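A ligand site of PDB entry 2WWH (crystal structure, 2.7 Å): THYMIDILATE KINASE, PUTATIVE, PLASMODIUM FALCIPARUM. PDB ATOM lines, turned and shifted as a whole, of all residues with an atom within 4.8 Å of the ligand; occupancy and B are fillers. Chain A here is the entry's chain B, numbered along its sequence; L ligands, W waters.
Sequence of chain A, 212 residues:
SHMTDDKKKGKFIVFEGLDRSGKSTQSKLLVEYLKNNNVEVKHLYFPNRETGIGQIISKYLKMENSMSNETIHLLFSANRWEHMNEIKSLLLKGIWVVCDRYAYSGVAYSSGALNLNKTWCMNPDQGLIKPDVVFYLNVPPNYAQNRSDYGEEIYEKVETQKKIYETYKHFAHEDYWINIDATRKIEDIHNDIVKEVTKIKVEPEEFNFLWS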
ATOM      1  N   LEU A  18       9.976  10.846 -27.857  1.00  0.00           N
ATOM      2  CA  LEU A  18       9.927  10.220 -29.186  1.00  0.00           C
ATOM      3  C   LEU A  18       8.585   9.539 -29.374  1.00  0.00           C
ATOM      4  O   LEU A  18       7.766   9.517 -28.471  1.00  0.00           O
ATOM      5  CB  LEU A  18      11.051   9.198 -29.371  1.00  0.00           C
ATOM      6  CG  LEU A  18      12.467   9.711 -29.625  1.00  0.00           C
ATOM      7  CD1 LEU A  18      13.387   8.553 -29.938  1.00  0.00           C
ATOM      8  CD2 LEU A  18      12.504  10.697 -30.729  1.00  0.00           C
ATOM      9  N   ASP A  19       8.363   9.007 -30.557  1.00  0.00           N
ATOM     10  CA  ASP A  19       7.048   8.479 -30.882  1.00  0.00           C
ATOM     11  C   ASP A  19       6.716   7.315 -29.988  1.00  0.00           C
ATOM     12  O   ASP A  19       7.567   6.468 -29.726  1.00  0.00           O
ATOM     13  CB  ASP A  19       6.987   8.060 -32.343  1.00  0.00           C
ATOM     14  CG  ASP A  19       6.679   9.213 -33.238  1.00  0.00           C
ATOM     15  OD1 ASP A  19       5.496   9.331 -33.670  1.00  0.00           O
ATOM     16  OD2 ASP A  19       7.601  10.018 -33.491  1.00  0.00           O
ATOM     17  N   ARG A  20       5.464   7.302 -29.523  1.00  0.00           N
ATOM     18  CA  ARG A  20       4.935   6.206 -28.713  1.00  0.00           C
ATOM     19  C   ARG A  20       5.597   6.101 -27.319  1.00  0.00           C
ATOM     20  O   ARG A  20       5.500   5.083 -26.658  1.00  0.00           O
ATOM     21  CB  ARG A  20       4.983   4.879 -29.502  1.00  0.00           C
ATOM     22  CG  ARG A  20       3.631   4.391 -30.076  1.00  0.00           C
ATOM     23  CD  ARG A  20       3.267   4.958 -31.466  1.00  0.00           C
ATOM     24  NE  ARG A  20       1.824   5.246 -31.585  1.00  0.00           N
ATOM     25  CZ  ARG A  20       1.118   5.324 -32.728  1.00  0.00           C
ATOM     26  NH1 ARG A  20       1.665   5.109 -33.925  1.00  0.00           N
ATOM     27  NH2 ARG A  20      -0.190   5.606 -32.661  1.00  0.00           N
ATOM     28  N   SER A  21       6.242   7.177 -26.867  1.00  0.00           N
ATOM     29  CA  SER A  21       7.063   7.104 -25.652  1.00  0.00           C
ATOM     30  C   SER A  21       6.316   7.149 -24.303  1.00  0.00           C
ATOM     31  O   SER A  21       6.953   7.088 -23.228  1.00  0.00           O
ATOM     32  CB  SER A  21       8.189   8.149 -25.698  1.00  0.00           C
ATOM     33  OG  SER A  21       7.686   9.422 -26.074  1.00  0.00           O
ATOM     34  N   GLY A  22       4.982   7.256 -24.342  1.00  0.00           N
ATOM     35  CA  GLY A  22       4.174   7.166 -23.124  1.00  0.00           C
ATOM     36  C   GLY A  22       3.613   8.489 -22.652  1.00  0.00           C
ATOM     37  O   GLY A  22       3.062   8.578 -21.535  1.00  0.00           O
ATOM     38  N   LYS A  23       3.713   9.501 -23.513  1.00  0.00           N
ATOM     39  CA  LYS A  23       3.210  10.861 -23.246  1.00  0.00           C
ATOM     40  C   LYS A  23       1.713  10.924 -22.957  1.00  0.00           C
ATOM     41  O   LYS A  23       1.335  11.550 -21.979  1.00  0.00           O
ATOM     42  CB  LYS A  23       3.585  11.828 -24.369  1.00  0.00           C
ATOM     43  CG  LYS A  23       5.068  11.986 -24.537  1.00  0.00           C
ATOM     44  CD  LYS A  23       5.437  13.070 -25.541  1.00  0.00           C
ATOM     45  CE  LYS A  23       5.751  12.498 -26.926  1.00  0.00           C
ATOM     46  NZ  LYS A  23       4.775  11.496 -27.424  1.00  0.00           N
ATOM     47  N   SER A  24       0.869  10.274 -23.747  1.00  0.00           N
ATOM     48  CA  SER A  24      -0.574  10.213 -23.389  1.00  0.00           C
ATOM     49  C   SER A  24      -0.778   9.443 -22.091  1.00  0.00           C
ATOM     50  O   SER A  24      -1.587   9.851 -21.241  1.00  0.00           O
ATOM     51  CB  SER A  24      -1.451   9.586 -24.489  1.00  0.00           C
ATOM     52  OG  SER A  24      -1.207  10.181 -25.763  1.00  0.00           O
ATOM     53  N   THR A  25      -0.028   8.354 -21.915  1.00  0.00           N
ATOM     54  CA  THR A  25      -0.165   7.513 -20.727  1.00  0.00           C
ATOM     55  C   THR A  25       0.142   8.312 -19.465  1.00  0.00           C
ATOM     56  O   THR A  25      -0.546   8.172 -18.436  1.00  0.00           O
ATOM     57  CB  THR A  25       0.779   6.303 -20.773  1.00  0.00           C
ATOM     58  OG1 THR A  25       0.479   5.471 -21.903  1.00  0.00           O
ATOM     59  CG2 THR A  25       0.616   5.479 -19.489  1.00  0.00           C
ATOM     60  N   PHE A  46      -0.528  18.635 -28.996  1.00  0.00           N
ATOM     61  CA  PHE A  46      -0.166  18.973 -30.385  1.00  0.00           C
ATOM     62  C   PHE A  46       0.412  17.771 -31.133  1.00  0.00           C
ATOM     63  O   PHE A  46       1.112  16.955 -30.544  1.00  0.00           O
ATOM     64  CB  PHE A  46       0.752  20.206 -30.451  1.00  0.00           C
ATOM     65  CG  PHE A  46       0.142  21.404 -29.831  1.00  0.00           C
ATOM     66  CD1 PHE A  46      -0.879  22.077 -30.481  1.00  0.00           C
ATOM     67  CD2 PHE A  46       0.520  21.808 -28.554  1.00  0.00           C
ATOM     68  CE1 PHE A  46      -1.498  23.154 -29.899  1.00  0.00           C
ATOM     69  CE2 PHE A  46      -0.090  22.891 -27.938  1.00  0.00           C
ATOM     70  CZ  PHE A  46      -1.107  23.573 -28.609  1.00  0.00           C
ATOM     71  N   PRO A  47       0.075  17.634 -32.421  1.00  0.00           N
ATOM     72  CA  PRO A  47      -0.838  18.558 -33.080  1.00  0.00           C
ATOM     73  C   PRO A  47      -2.278  18.285 -32.688  1.00  0.00           C
ATOM     74  O   PRO A  47      -2.649  17.138 -32.371  1.00  0.00           O
ATOM     75  CB  PRO A  47      -0.647  18.244 -34.565  1.00  0.00           C
ATOM     76  CG  PRO A  47      -0.292  16.830 -34.605  1.00  0.00           C
ATOM     77  CD  PRO A  47       0.520  16.556 -33.329  1.00  0.00           C
ATOM     78  N   ARG A  49      -5.483  17.860 -34.286  1.00  0.00           N
ATOM     79  CA  ARG A  49      -5.898  17.452 -35.607  1.00  0.00           C
ATOM     80  C   ARG A  49      -7.357  17.802 -35.926  1.00  0.00           C
ATOM     81  O   ARG A  49      -7.889  17.386 -36.959  1.00  0.00           O
ATOM     82  CB  ARG A  49      -5.675  15.953 -35.741  1.00  0.00           C
ATOM     83  CG  ARG A  49      -4.362  15.470 -35.169  1.00  0.00           C
ATOM     84  CD  ARG A  49      -4.117  14.108 -35.707  1.00  0.00           C
ATOM     85  NE  ARG A  49      -2.965  13.412 -35.136  1.00  0.00           N
ATOM     86  CZ  ARG A  49      -2.370  12.368 -35.739  1.00  0.00           C
ATOM     87  NH1 ARG A  49      -2.816  11.941 -36.921  1.00  0.00           N
ATOM     88  NH2 ARG A  49      -1.331  11.761 -35.160  1.00  0.00           N
ATOM     89  N   LEU A  61       0.607  13.419 -41.642  1.00  0.00           N
ATOM     90  CA  LEU A  61       1.152  12.379 -40.766  1.00  0.00           C
ATOM     91  C   LEU A  61       0.751  10.969 -41.187  1.00  0.00           C
ATOM     92  O   LEU A  61       1.542  10.037 -41.070  1.00  0.00           O
ATOM     93  CB  LEU A  61       0.738  12.619 -39.301  1.00  0.00           C
ATOM     94  CG  LEU A  61       1.375  13.810 -38.594  1.00  0.00           C
ATOM     95  CD1 LEU A  61       0.786  13.957 -37.216  1.00  0.00           C
ATOM     96  CD2 LEU A  61       2.905  13.711 -38.529  1.00  0.00           C
ATOM     97  N   PHE A  76       2.635  23.080 -38.241  1.00  0.00           N
ATOM     98  CA  PHE A  76       2.794  22.600 -36.864  1.00  0.00           C
ATOM     99  C   PHE A  76       2.887  23.740 -35.856  1.00  0.00           C
ATOM    100  O   PHE A  76       2.422  23.636 -34.708  1.00  0.00           O
ATOM    101  CB  PHE A  76       4.054  21.775 -36.736  1.00  0.00           C
ATOM    102  CG  PHE A  76       3.872  20.343 -37.080  1.00  0.00           C
ATOM    103  CD1 PHE A  76       3.038  19.535 -36.308  1.00  0.00           C
ATOM    104  CD2 PHE A  76       4.582  19.782 -38.126  1.00  0.00           C
ATOM    105  CE1 PHE A  76       2.893  18.190 -36.601  1.00  0.00           C
ATOM    106  CE2 PHE A  76       4.428  18.443 -38.433  1.00  0.00           C
ATOM    107  CZ  PHE A  76       3.581  17.652 -37.666  1.00  0.00           C
ATOM    108  N   ARG A  80      -0.019  25.611 -32.927  1.00  0.00           N
ATOM    109  CA  ARG A  80       0.242  26.030 -31.575  1.00  0.00           C
ATOM    110  C   ARG A  80      -0.239  27.450 -31.357  1.00  0.00           C
ATOM    111  O   ARG A  80      -0.749  27.760 -30.280  1.00  0.00           O
ATOM    112  CB  ARG A  80       1.734  25.892 -31.267  1.00  0.00           C
ATOM    113  CG  ARG A  80       2.185  24.459 -30.996  1.00  0.00           C
ATOM    114  CD  ARG A  80       3.661  24.365 -30.643  1.00  0.00           C
ATOM    115  NE  ARG A  80       4.560  24.516 -31.791  1.00  0.00           N
ATOM    116  CZ  ARG A  80       4.833  23.512 -32.636  1.00  0.00           C
ATOM    117  NH1 ARG A  80       4.198  22.334 -32.484  1.00  0.00           N
ATOM    118  NH2 ARG A  80       5.681  23.690 -33.654  1.00  0.00           N
ATOM    119  N   ASP A 100       0.651  17.743 -24.055  1.00  0.00           N
ATOM    120  CA  ASP A 100       1.367  16.678 -24.709  1.00  0.00           C
ATOM    121  C   ASP A 100       1.927  17.192 -26.049  1.00  0.00           C
ATOM    122  O   ASP A 100       1.171  17.409 -26.994  1.00  0.00           O
ATOM    123  CB  ASP A 100       0.388  15.538 -24.924  1.00  0.00           C
ATOM    124  CG  ASP A 100       0.966  14.401 -25.729  1.00  0.00           C
ATOM    125  OD1 ASP A 100       1.991  14.579 -26.430  1.00  0.00           O
ATOM    126  OD2 ASP A 100       0.356  13.298 -25.678  1.00  0.00           O
ATOM    127  N   ARG A 101       3.252  17.350 -26.103  1.00  0.00           N
ATOM    128  CA  ARG A 101       4.023  17.909 -27.233  1.00  0.00           C
ATOM    129  C   ARG A 101       3.890  19.415 -27.344  1.00  0.00           C
ATOM    130  O   ARG A 101       2.880  19.968 -26.922  1.00  0.00           O
ATOM    131  CB  ARG A 101       3.697  17.248 -28.583  1.00  0.00           C
ATOM    132  CG  ARG A 101       3.966  15.766 -28.671  1.00  0.00           C
ATOM    133  CD  ARG A 101       4.500  15.415 -30.013  1.00  0.00           C
ATOM    134  NE  ARG A 101       4.609  13.980 -30.180  1.00  0.00           N
ATOM    135  CZ  ARG A 101       5.769  13.319 -30.277  1.00  0.00           C
ATOM    136  NH1 ARG A 101       6.938  13.972 -30.233  1.00  0.00           N
ATOM    137  NH2 ARG A 101       5.766  12.004 -30.437  1.00  0.00           N
ATOM    138  N   TYR A 102       4.914  20.035 -27.911  1.00  0.00           N
ATOM    139  CA  TYR A 102       5.031  21.469 -28.058  1.00  0.00           C
ATOM    140  C   TYR A 102       6.125  21.877 -29.087  1.00  0.00           C
ATOM    141  O   TYR A 102       6.551  21.072 -29.932  1.00  0.00           O
ATOM    142  CB  TYR A 102       5.347  22.086 -26.708  1.00  0.00           C
ATOM    143  CG  TYR A 102       4.801  23.495 -26.544  1.00  0.00           C
ATOM    144  CD1 TYR A 102       3.467  23.794 -26.838  1.00  0.00           C
ATOM    145  CD2 TYR A 102       5.607  24.517 -26.076  1.00  0.00           C
ATOM    146  CE1 TYR A 102       2.966  25.055 -26.692  1.00  0.00           C
ATOM    147  CE2 TYR A 102       5.112  25.781 -25.917  1.00  0.00           C
ATOM    148  CZ  TYR A 102       3.792  26.050 -26.225  1.00  0.00           C
ATOM    149  OH  TYR A 102       3.314  27.343 -26.042  1.00  0.00           O
ATOM    150  N   SER A 105       9.097  19.340 -29.950  1.00  0.00           N
ATOM    151  CA  SER A 105       8.644  18.431 -31.013  1.00  0.00           C
ATOM    152  C   SER A 105       8.858  19.067 -32.396  1.00  0.00           C
ATOM    153  O   SER A 105       9.441  18.439 -33.270  1.00  0.00           O
ATOM    154  CB  SER A 105       7.149  18.078 -30.816  1.00  0.00           C
ATOM    155  OG  SER A 105       6.961  17.028 -29.857  1.00  0.00           O
ATOM    156  N   GLY A 106       8.408  20.310 -32.549  1.00  0.00           N
ATOM    157  CA  GLY A 106       8.517  21.044 -33.794  1.00  0.00           C
ATOM    158  C   GLY A 106       9.955  21.108 -34.270  1.00  0.00           C
ATOM    159  O   GLY A 106      10.267  20.784 -35.426  1.00  0.00           O
ATOM    160  N   TYR A 109      11.751  17.191 -34.502  1.00  0.00           N
ATOM    161  CA  TYR A 109      11.264  16.498 -35.673  1.00  0.00           C
ATOM    162  C   TYR A 109      11.733  17.086 -36.996  1.00  0.00           C
ATOM    163  O   TYR A 109      12.195  16.380 -37.866  1.00  0.00           O
ATOM    164  CB  TYR A 109       9.743  16.360 -35.604  1.00  0.00           C
ATOM    165  CG  TYR A 109       9.411  15.228 -34.701  1.00  0.00           C
ATOM    166  CD1 TYR A 109       9.063  13.996 -35.199  1.00  0.00           C
ATOM    167  CD2 TYR A 109       9.565  15.358 -33.317  1.00  0.00           C
ATOM    168  CE1 TYR A 109       8.833  12.939 -34.371  1.00  0.00           C
ATOM    169  CE2 TYR A 109       9.329  14.302 -32.470  1.00  0.00           C
ATOM    170  CZ  TYR A 109       8.963  13.093 -32.997  1.00  0.00           C
ATOM    171  OH  TYR A 109       8.709  12.046 -32.135  1.00  0.00           O
ATOM    172  N   ARG A 147       6.434  -0.713 -29.685  1.00  0.00           N
ATOM    173  CA  ARG A 147       5.171  -0.075 -29.357  1.00  0.00           C
ATOM    174  C   ARG A 147       4.047  -0.634 -30.229  1.00  0.00           C
ATOM    175  O   ARG A 147       4.298  -1.120 -31.334  1.00  0.00           O
ATOM    176  CB  ARG A 147       5.265   1.442 -29.538  1.00  0.00           C
ATOM    177  CG  ARG A 147       5.611   2.201 -28.260  1.00  0.00           C
ATOM    178  CD  ARG A 147       5.637   1.273 -27.063  1.00  0.00           C
ATOM    179  NE  ARG A 147       5.515   2.007 -25.800  1.00  0.00           N
ATOM    180  CZ  ARG A 147       6.418   1.980 -24.834  1.00  0.00           C
ATOM    181  NH1 ARG A 147       6.217   2.675 -23.724  1.00  0.00           N
ATOM    182  NH2 ARG A 147       7.522   1.250 -24.969  1.00  0.00           N
ATOM    183  N   SER A 148       2.826  -0.582 -29.715  1.00  0.00           N
ATOM    184  CA  SER A 148       1.665  -1.202 -30.363  1.00  0.00           C
ATOM    185  C   SER A 148       1.293  -0.743 -31.771  1.00  0.00           C
ATOM    186  O   SER A 148       0.978  -1.600 -32.608  1.00  0.00           O
ATOM    187  CB  SER A 148       0.435  -1.088 -29.453  1.00  0.00           C
ATOM    188  OG  SER A 148       0.162  -2.314 -28.811  1.00  0.00           O
ATOM    189  N   GLU A 153       2.405   5.813 -38.884  1.00  0.00           N
ATOM    190  CA  GLU A 153       2.528   7.240 -39.239  1.00  0.00           C
ATOM    191  C   GLU A 153       3.927   7.665 -39.665  1.00  0.00           C
ATOM    192  O   GLU A 153       4.906   6.955 -39.441  1.00  0.00           O
ATOM    193  CB  GLU A 153       1.964   8.148 -38.162  1.00  0.00           C
ATOM    194  CG  GLU A 153       0.441   8.117 -38.142  1.00  0.00           C
ATOM    195  CD  GLU A 153      -0.160   9.141 -37.212  1.00  0.00           C
ATOM    196  OE1 GLU A 153       0.618   9.876 -36.524  1.00  0.00           O
ATOM    197  OE2 GLU A 153      -1.416   9.193 -37.177  1.00  0.00           O
ATOM    198  N   TYR A 155       6.716   9.267 -39.372  1.00  0.00           N
ATOM    199  CA  TYR A 155       8.056   9.390 -38.793  1.00  0.00           C
ATOM    200  C   TYR A 155       8.501   8.159 -38.016  1.00  0.00           C
ATOM    201  O   TYR A 155       9.699   8.017 -37.705  1.00  0.00           O
ATOM    202  CB  TYR A 155       8.142  10.617 -37.898  1.00  0.00           C
ATOM    203  CG  TYR A 155       8.120  11.929 -38.638  1.00  0.00           C
ATOM    204  CD1 TYR A 155       8.963  12.159 -39.714  1.00  0.00           C
ATOM    205  CD2 TYR A 155       7.279  12.953 -38.227  1.00  0.00           C
ATOM    206  CE1 TYR A 155       8.950  13.376 -40.403  1.00  0.00           C
ATOM    207  CE2 TYR A 155       7.264  14.192 -38.896  1.00  0.00           C
ATOM    208  CZ  TYR A 155       8.096  14.398 -39.985  1.00  0.00           C
ATOM    209  OH  TYR A 155       8.087  15.613 -40.620  1.00  0.00           O
ATOM    210  N   GLU A 156       7.524   7.296 -37.715  1.00  0.00           N
ATOM    211  CA  GLU A 156       7.718   6.070 -36.941  1.00  0.00           C
ATOM    212  C   GLU A 156       8.459   5.002 -37.735  1.00  0.00           C
ATOM    213  O   GLU A 156       7.872   3.975 -38.074  1.00  0.00           O
ATOM    214  CB  GLU A 156       6.359   5.511 -36.430  1.00  0.00           C
ATOM    215  CG  GLU A 156       5.389   6.608 -35.952  1.00  0.00           C
ATOM    216  CD  GLU A 156       4.171   6.104 -35.193  1.00  0.00           C
ATOM    217  OE1 GLU A 156       3.686   4.984 -35.470  1.00  0.00           O
ATOM    218  OE2 GLU A 156       3.686   6.861 -34.292  1.00  0.00           O
ATOM    219  N   ALA A 182      12.200   6.786 -19.271  1.00  0.00           N
ATOM    220  CA  ALA A 182      10.797   6.393 -19.443  1.00  0.00           C
ATOM    221  C   ALA A 182      10.592   4.930 -19.825  1.00  0.00           C
ATOM    222  O   ALA A 182       9.466   4.539 -20.144  1.00  0.00           O
ATOM    223  CB  ALA A 182      10.113   7.298 -20.477  1.00  0.00           C
ATOM    224  N   ARG A 184      10.172   2.182 -18.193  1.00  0.00           N
ATOM    225  CA  ARG A 184       9.932   1.590 -16.896  1.00  0.00           C
ATOM    226  C   ARG A 184       8.506   1.032 -16.643  1.00  0.00           C
ATOM    227  O   ARG A 184       7.731   0.751 -17.578  1.00  0.00           O
ATOM    228  CB  ARG A 184      10.383   2.567 -15.785  1.00  0.00           C
ATOM    229  CG  ARG A 184      11.894   2.583 -15.596  1.00  0.00           C
ATOM    230  CD  ARG A 184      12.306   3.295 -14.314  1.00  0.00           C
ATOM    231  NE  ARG A 184      12.437   4.736 -14.509  1.00  0.00           N
ATOM    232  CZ  ARG A 184      12.240   5.648 -13.558  1.00  0.00           C
ATOM    233  NH1 ARG A 184      11.911   5.287 -12.316  1.00  0.00           N
ATOM    234  NH2 ARG A 184      12.378   6.943 -13.848  1.00  0.00           N
ATOM    235  N   LYS A 185       8.194   0.814 -15.371  1.00  0.00           N
ATOM    236  CA  LYS A 185       6.811   0.557 -15.034  1.00  0.00           C
ATOM    237  C   LYS A 185       6.153   1.939 -15.035  1.00  0.00           C
ATOM    238  O   LYS A 185       6.652   2.905 -14.385  1.00  0.00           O
ATOM    239  CB  LYS A 185       6.662  -0.197 -13.717  1.00  0.00           C
ATOM    240  CG  LYS A 185       7.023  -1.672 -13.826  1.00  0.00           C
ATOM    241  CD  LYS A 185       5.886  -2.550 -13.294  1.00  0.00           C
ATOM    242  CE  LYS A 185       5.982  -2.748 -11.795  1.00  0.00           C
ATOM    243  NZ  LYS A 185       7.123  -3.684 -11.449  1.00  0.00           N
ATOM    244  N   ILE A 186       5.082   2.035 -15.819  1.00  0.00           N
ATOM    245  CA  ILE A 186       4.253   3.222 -15.901  1.00  0.00           C
ATOM    246  C   ILE A 186       4.228   3.918 -14.538  1.00  0.00           C
ATOM    247  O   ILE A 186       4.535   5.117 -14.445  1.00  0.00           O
ATOM    248  CB  ILE A 186       2.848   2.841 -16.436  1.00  0.00           C
ATOM    249  CG1 ILE A 186       2.933   2.463 -17.912  1.00  0.00           C
ATOM    250  CG2 ILE A 186       1.846   3.983 -16.257  1.00  0.00           C
ATOM    251  CD1 ILE A 186       1.752   1.649 -18.439  1.00  0.00           C
ATOM    252  N   ILE A 189       7.509   5.879 -13.340  1.00  0.00           N
ATOM    253  CA  ILE A 189       7.642   7.133 -14.075  1.00  0.00           C
ATOM    254  C   ILE A 189       6.685   8.119 -13.448  1.00  0.00           C
ATOM    255  O   ILE A 189       7.059   9.243 -13.104  1.00  0.00           O
ATOM    256  CB  ILE A 189       7.295   6.979 -15.546  1.00  0.00           C
ATOM    257  CG1 ILE A 189       8.339   6.127 -16.247  1.00  0.00           C
ATOM    258  CG2 ILE A 189       7.297   8.315 -16.216  1.00  0.00           C
ATOM    259  CD1 ILE A 189       7.805   5.454 -17.489  1.00  0.00           C
HETATM  260  N1  LIG L   1       5.286  16.440 -34.815  1.00  0.00           N
HETATM  261  C1  LIG L   1       4.553  16.901 -33.782  1.00  0.00           C
HETATM  262  C2  LIG L   1       6.079  17.344 -35.575  1.00  0.00           C
HETATM  263  O1  LIG L   1       6.758  16.934 -36.523  1.00  0.00           O
HETATM  264  N2  LIG L   1       6.113  18.650 -35.307  1.00  0.00           N
HETATM  265  C3  LIG L   1       5.414  19.136 -34.296  1.00  0.00           C
HETATM  266  O2  LIG L   1       5.438  20.344 -34.048  1.00  0.00           O
HETATM  267  C4  LIG L   1       4.569  18.260 -33.471  1.00  0.00           C
HETATM  268  C5  LIG L   1       3.767  18.803 -32.329  1.00  0.00           C
HETATM  269  C6  LIG L   1       2.572  12.514 -34.450  1.00  0.00           C
HETATM  270  C7  LIG L   1       3.889  13.099 -34.924  1.00  0.00           C
HETATM  271  O3  LIG L   1       3.886  14.505 -35.079  1.00  0.00           O
HETATM  272  C8  LIG L   1       5.236  14.982 -35.110  1.00  0.00           C
HETATM  273  C9  LIG L   1       5.819  14.171 -33.979  1.00  0.00           C
HETATM  274  C10 LIG L   1       5.101  12.838 -34.071  1.00  0.00           C
HETATM  275  O4  LIG L   1       5.915  11.965 -34.850  1.00  0.00           O
HETATM  276  P1  LIG L   1       1.594  12.103 -32.043  1.00  0.00           P
HETATM  277  O5  LIG L   1       0.275  11.474 -32.342  1.00  0.00           O
HETATM  278  O6  LIG L   1       1.662  12.969 -30.805  1.00  0.00           O
HETATM  279  O7  LIG L   1       2.119  13.074 -33.229  1.00  0.00           O
HETATM  280  O8  LIG L   1       2.742  10.949 -32.095  1.00  0.00           O
HETATM  281  P2  LIG L   1       3.065   9.923 -30.894  1.00  0.00           P
HETATM  282  O9  LIG L   1       4.087   8.901 -31.295  1.00  0.00           O
HETATM  283  O10 LIG L   1       3.288  10.723 -29.641  1.00  0.00           O
HETATM  284  O11 LIG L   1       1.710   9.107 -30.835  1.00  0.00           O
HETATM  285  P3  LIG L   1       1.148   8.807 -29.370  1.00  0.00           P
HETATM  286  O12 LIG L   1       0.276   7.596 -29.522  1.00  0.00           O
HETATM  287  O13 LIG L   1       0.498  10.104 -28.939  1.00  0.00           O
HETATM  288  O14 LIG L   1       2.440   8.408 -28.449  1.00  0.00           O
HETATM  289  P4  LIG L   1       2.515   8.440 -26.812  1.00  0.00           P
HETATM  290  O15 LIG L   1       3.892   8.926 -26.442  1.00  0.00           O
HETATM  291  O16 LIG L   1       1.288   9.134 -26.284  1.00  0.00           O
HETATM  292  O17 LIG L   1       2.411   6.914 -26.306  1.00  0.00           O
HETATM  293  P5  LIG L   1       1.176   6.352 -25.412  1.00  0.00           P
HETATM  294  O18 LIG L   1      -0.100   6.411 -26.202  1.00  0.00           O
HETATM  295  O19 LIG L   1       1.208   7.009 -24.059  1.00  0.00           O
HETATM  296  O20 LIG L   1       1.593   4.809 -25.210  1.00  0.00           O
HETATM  297  C11 LIG L   1       2.011   3.932 -26.267  1.00  0.00           C
HETATM  298  C12 LIG L   1       1.801   2.490 -25.802  1.00  0.00           C
HETATM  299  O21 LIG L   1       2.767   2.161 -24.809  1.00  0.00           O
HETATM  300  C13 LIG L   1       2.167   1.777 -23.586  1.00  0.00           C
HETATM  301  C14 LIG L   1       0.831   2.467 -23.668  1.00  0.00           C
HETATM  302  O22 LIG L   1      -0.160   1.984 -22.757  1.00  0.00           O
HETATM  303  C15 LIG L   1       0.472   2.250 -25.119  1.00  0.00           C
HETATM  304  O23 LIG L   1       0.109   0.906 -25.350  1.00  0.00           O
HETATM  305  N3  LIG L   1       3.035   2.316 -22.516  1.00  0.00           N
HETATM  306  C16 LIG L   1       4.015   1.639 -21.901  1.00  0.00           C
HETATM  307  N4  LIG L   1       4.487   0.374 -22.025  1.00  0.00           N
HETATM  308  C17 LIG L   1       5.507  -0.045 -21.251  1.00  0.00           C
HETATM  309  N5  LIG L   1       6.084   0.757 -20.341  1.00  0.00           N
HETATM  310  C18 LIG L   1       5.651   2.036 -20.183  1.00  0.00           C
HETATM  311  N6  LIG L   1       6.235   2.850 -19.271  1.00  0.00           N
HETATM  312  C19 LIG L   1       4.592   2.495 -20.972  1.00  0.00           C
HETATM  313  N7  LIG L   1       3.939   3.681 -21.056  1.00  0.00           N
HETATM  314  C20 LIG L   1       2.997   3.545 -22.005  1.00  0.00           C
HETATM  315  O   HOH W   1       3.223   9.565 -35.010  1.00  0.00           O
HETATM  316  O   HOH W   2      -2.638   8.625 -28.129  1.00  0.00           O
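O19 of the ligand is in hydrogen-bond range of N of Thr 25 (2.8 Å). The side-chain hydroxyl (OG1) of Thr 25 lies within hydrogen-bond range of an oxygen (O19) of the ligand, at 2.7 Å. N of Arg 20 lies within hydrogen-bond range of O9 of the ligand, 2.8 Å away. NE of Arg 20 is in salt-bridge range of O12 of the ligand, 3.5 Å away. N of Ser 24 is in hydrogen-bond range of O16 of the ligand (2.8 Å). An oxygen (O16) of the ligand sits at hydrogen-bond distance from the side-chain hydroxyl (OG) of Ser 24 (2.8 Å). An oxygen (O15) of the ligand lies within hydrogen-bond range of the backbone NH (N) of Lys 23, 3.0 Å away. The side-chain amino group (NZ) of Lys 23 lies within salt-bridge range of an oxygen (O10) of the ligand (2.8 Å). OD2 of Asp 19 is in hydrogen-bond range of O4 of the ligand (2.9 Å). The guanidinium group of Arg 80 sits at hydrogen-bond distance from an oxygen (O2) of the ligand (2.8 Å). An oxygen (O15) of the ligand sits at hydrogen-bond distance from the backbone NH (N) of Gly 22 (2.9 Å). An oxygen (O10) of the ligand lies within salt-bridge range of the guanidinium group of Arg 101 (2.9 Å). The guanidinium group (NE) of Arg 147 is in hydrogen-bond range of an oxygen (O21) of the ligand (2.9 Å). The backbone NH (N) of Ser 21 is in hydrogen-bond range of an oxygen (O15) of the ligand (3.0 Å). The backbone carbonyl oxygen (O) of Arg 184 sits at hydrogen-bond distance from a nitrogen (N6) of the ligand (3.1 Å). The backbone NH of Gly 106 sits close to an oxygen (O2) of the ligand. The guanidinium group (NH2) of Arg 49 is in salt-bridge range of an oxygen (O5) of the ligand (3.3 Å).
Water W2 lies within hydrogen-bond range of OG of Ser 24 (3.2 Å) and O12 of the ligand (3.4 Å).
Residues that only touch the ligand: Tyr 109, Phe 76, Ile 186, Ile 189, Leu 61, Glu 156, Tyr 155, Phe 46, Ser 105, Ala 182, Pro 47 and Glu 153. Hydrophobic or aromatic side chains within 4 Å of the ligand: Phe 46, Pro 47, Leu 61, Phe 76, Tyr 109, Tyr 155, Ile 186 and Ile 189.
The backbone carbonyl oxygen (O) of Arg 20 lies within hydrogen-bond range of the guanidinium group (NE) of Arg 147 (3.2 Å). OE1 of Glu 156 lies within salt-bridge range of NH1 of Arg 20 (2.5 Å). The side-chain hydroxyl (OG) of Ser 24 is in hydrogen-bond range of the side-chain carboxylate (OD2) of Asp 100 (3.5 Å). NH1 of Arg 80 lies within hydrogen-bond range of O of Phe 76 (3.1 Å). The guanidinium group (NH1) of Arg 101 sits at hydrogen-bond distance from the side-chain hydroxyl (OH) of Tyr 109 (3.2 Å). The side-chain hydroxyl (OG) of Ser 105 lies close to the guanidinium group (NH1) of Arg 101, at 3.1 Å. The side-chain carboxylate (OE1) of Glu 153 is in salt-bridge range of the guanidinium group (NH2) of Arg 49 (3.0 Å). The backbone NH (N) of Phe 46 is in hydrogen-bond range of the backbone carbonyl oxygen (O) of Asp 100.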
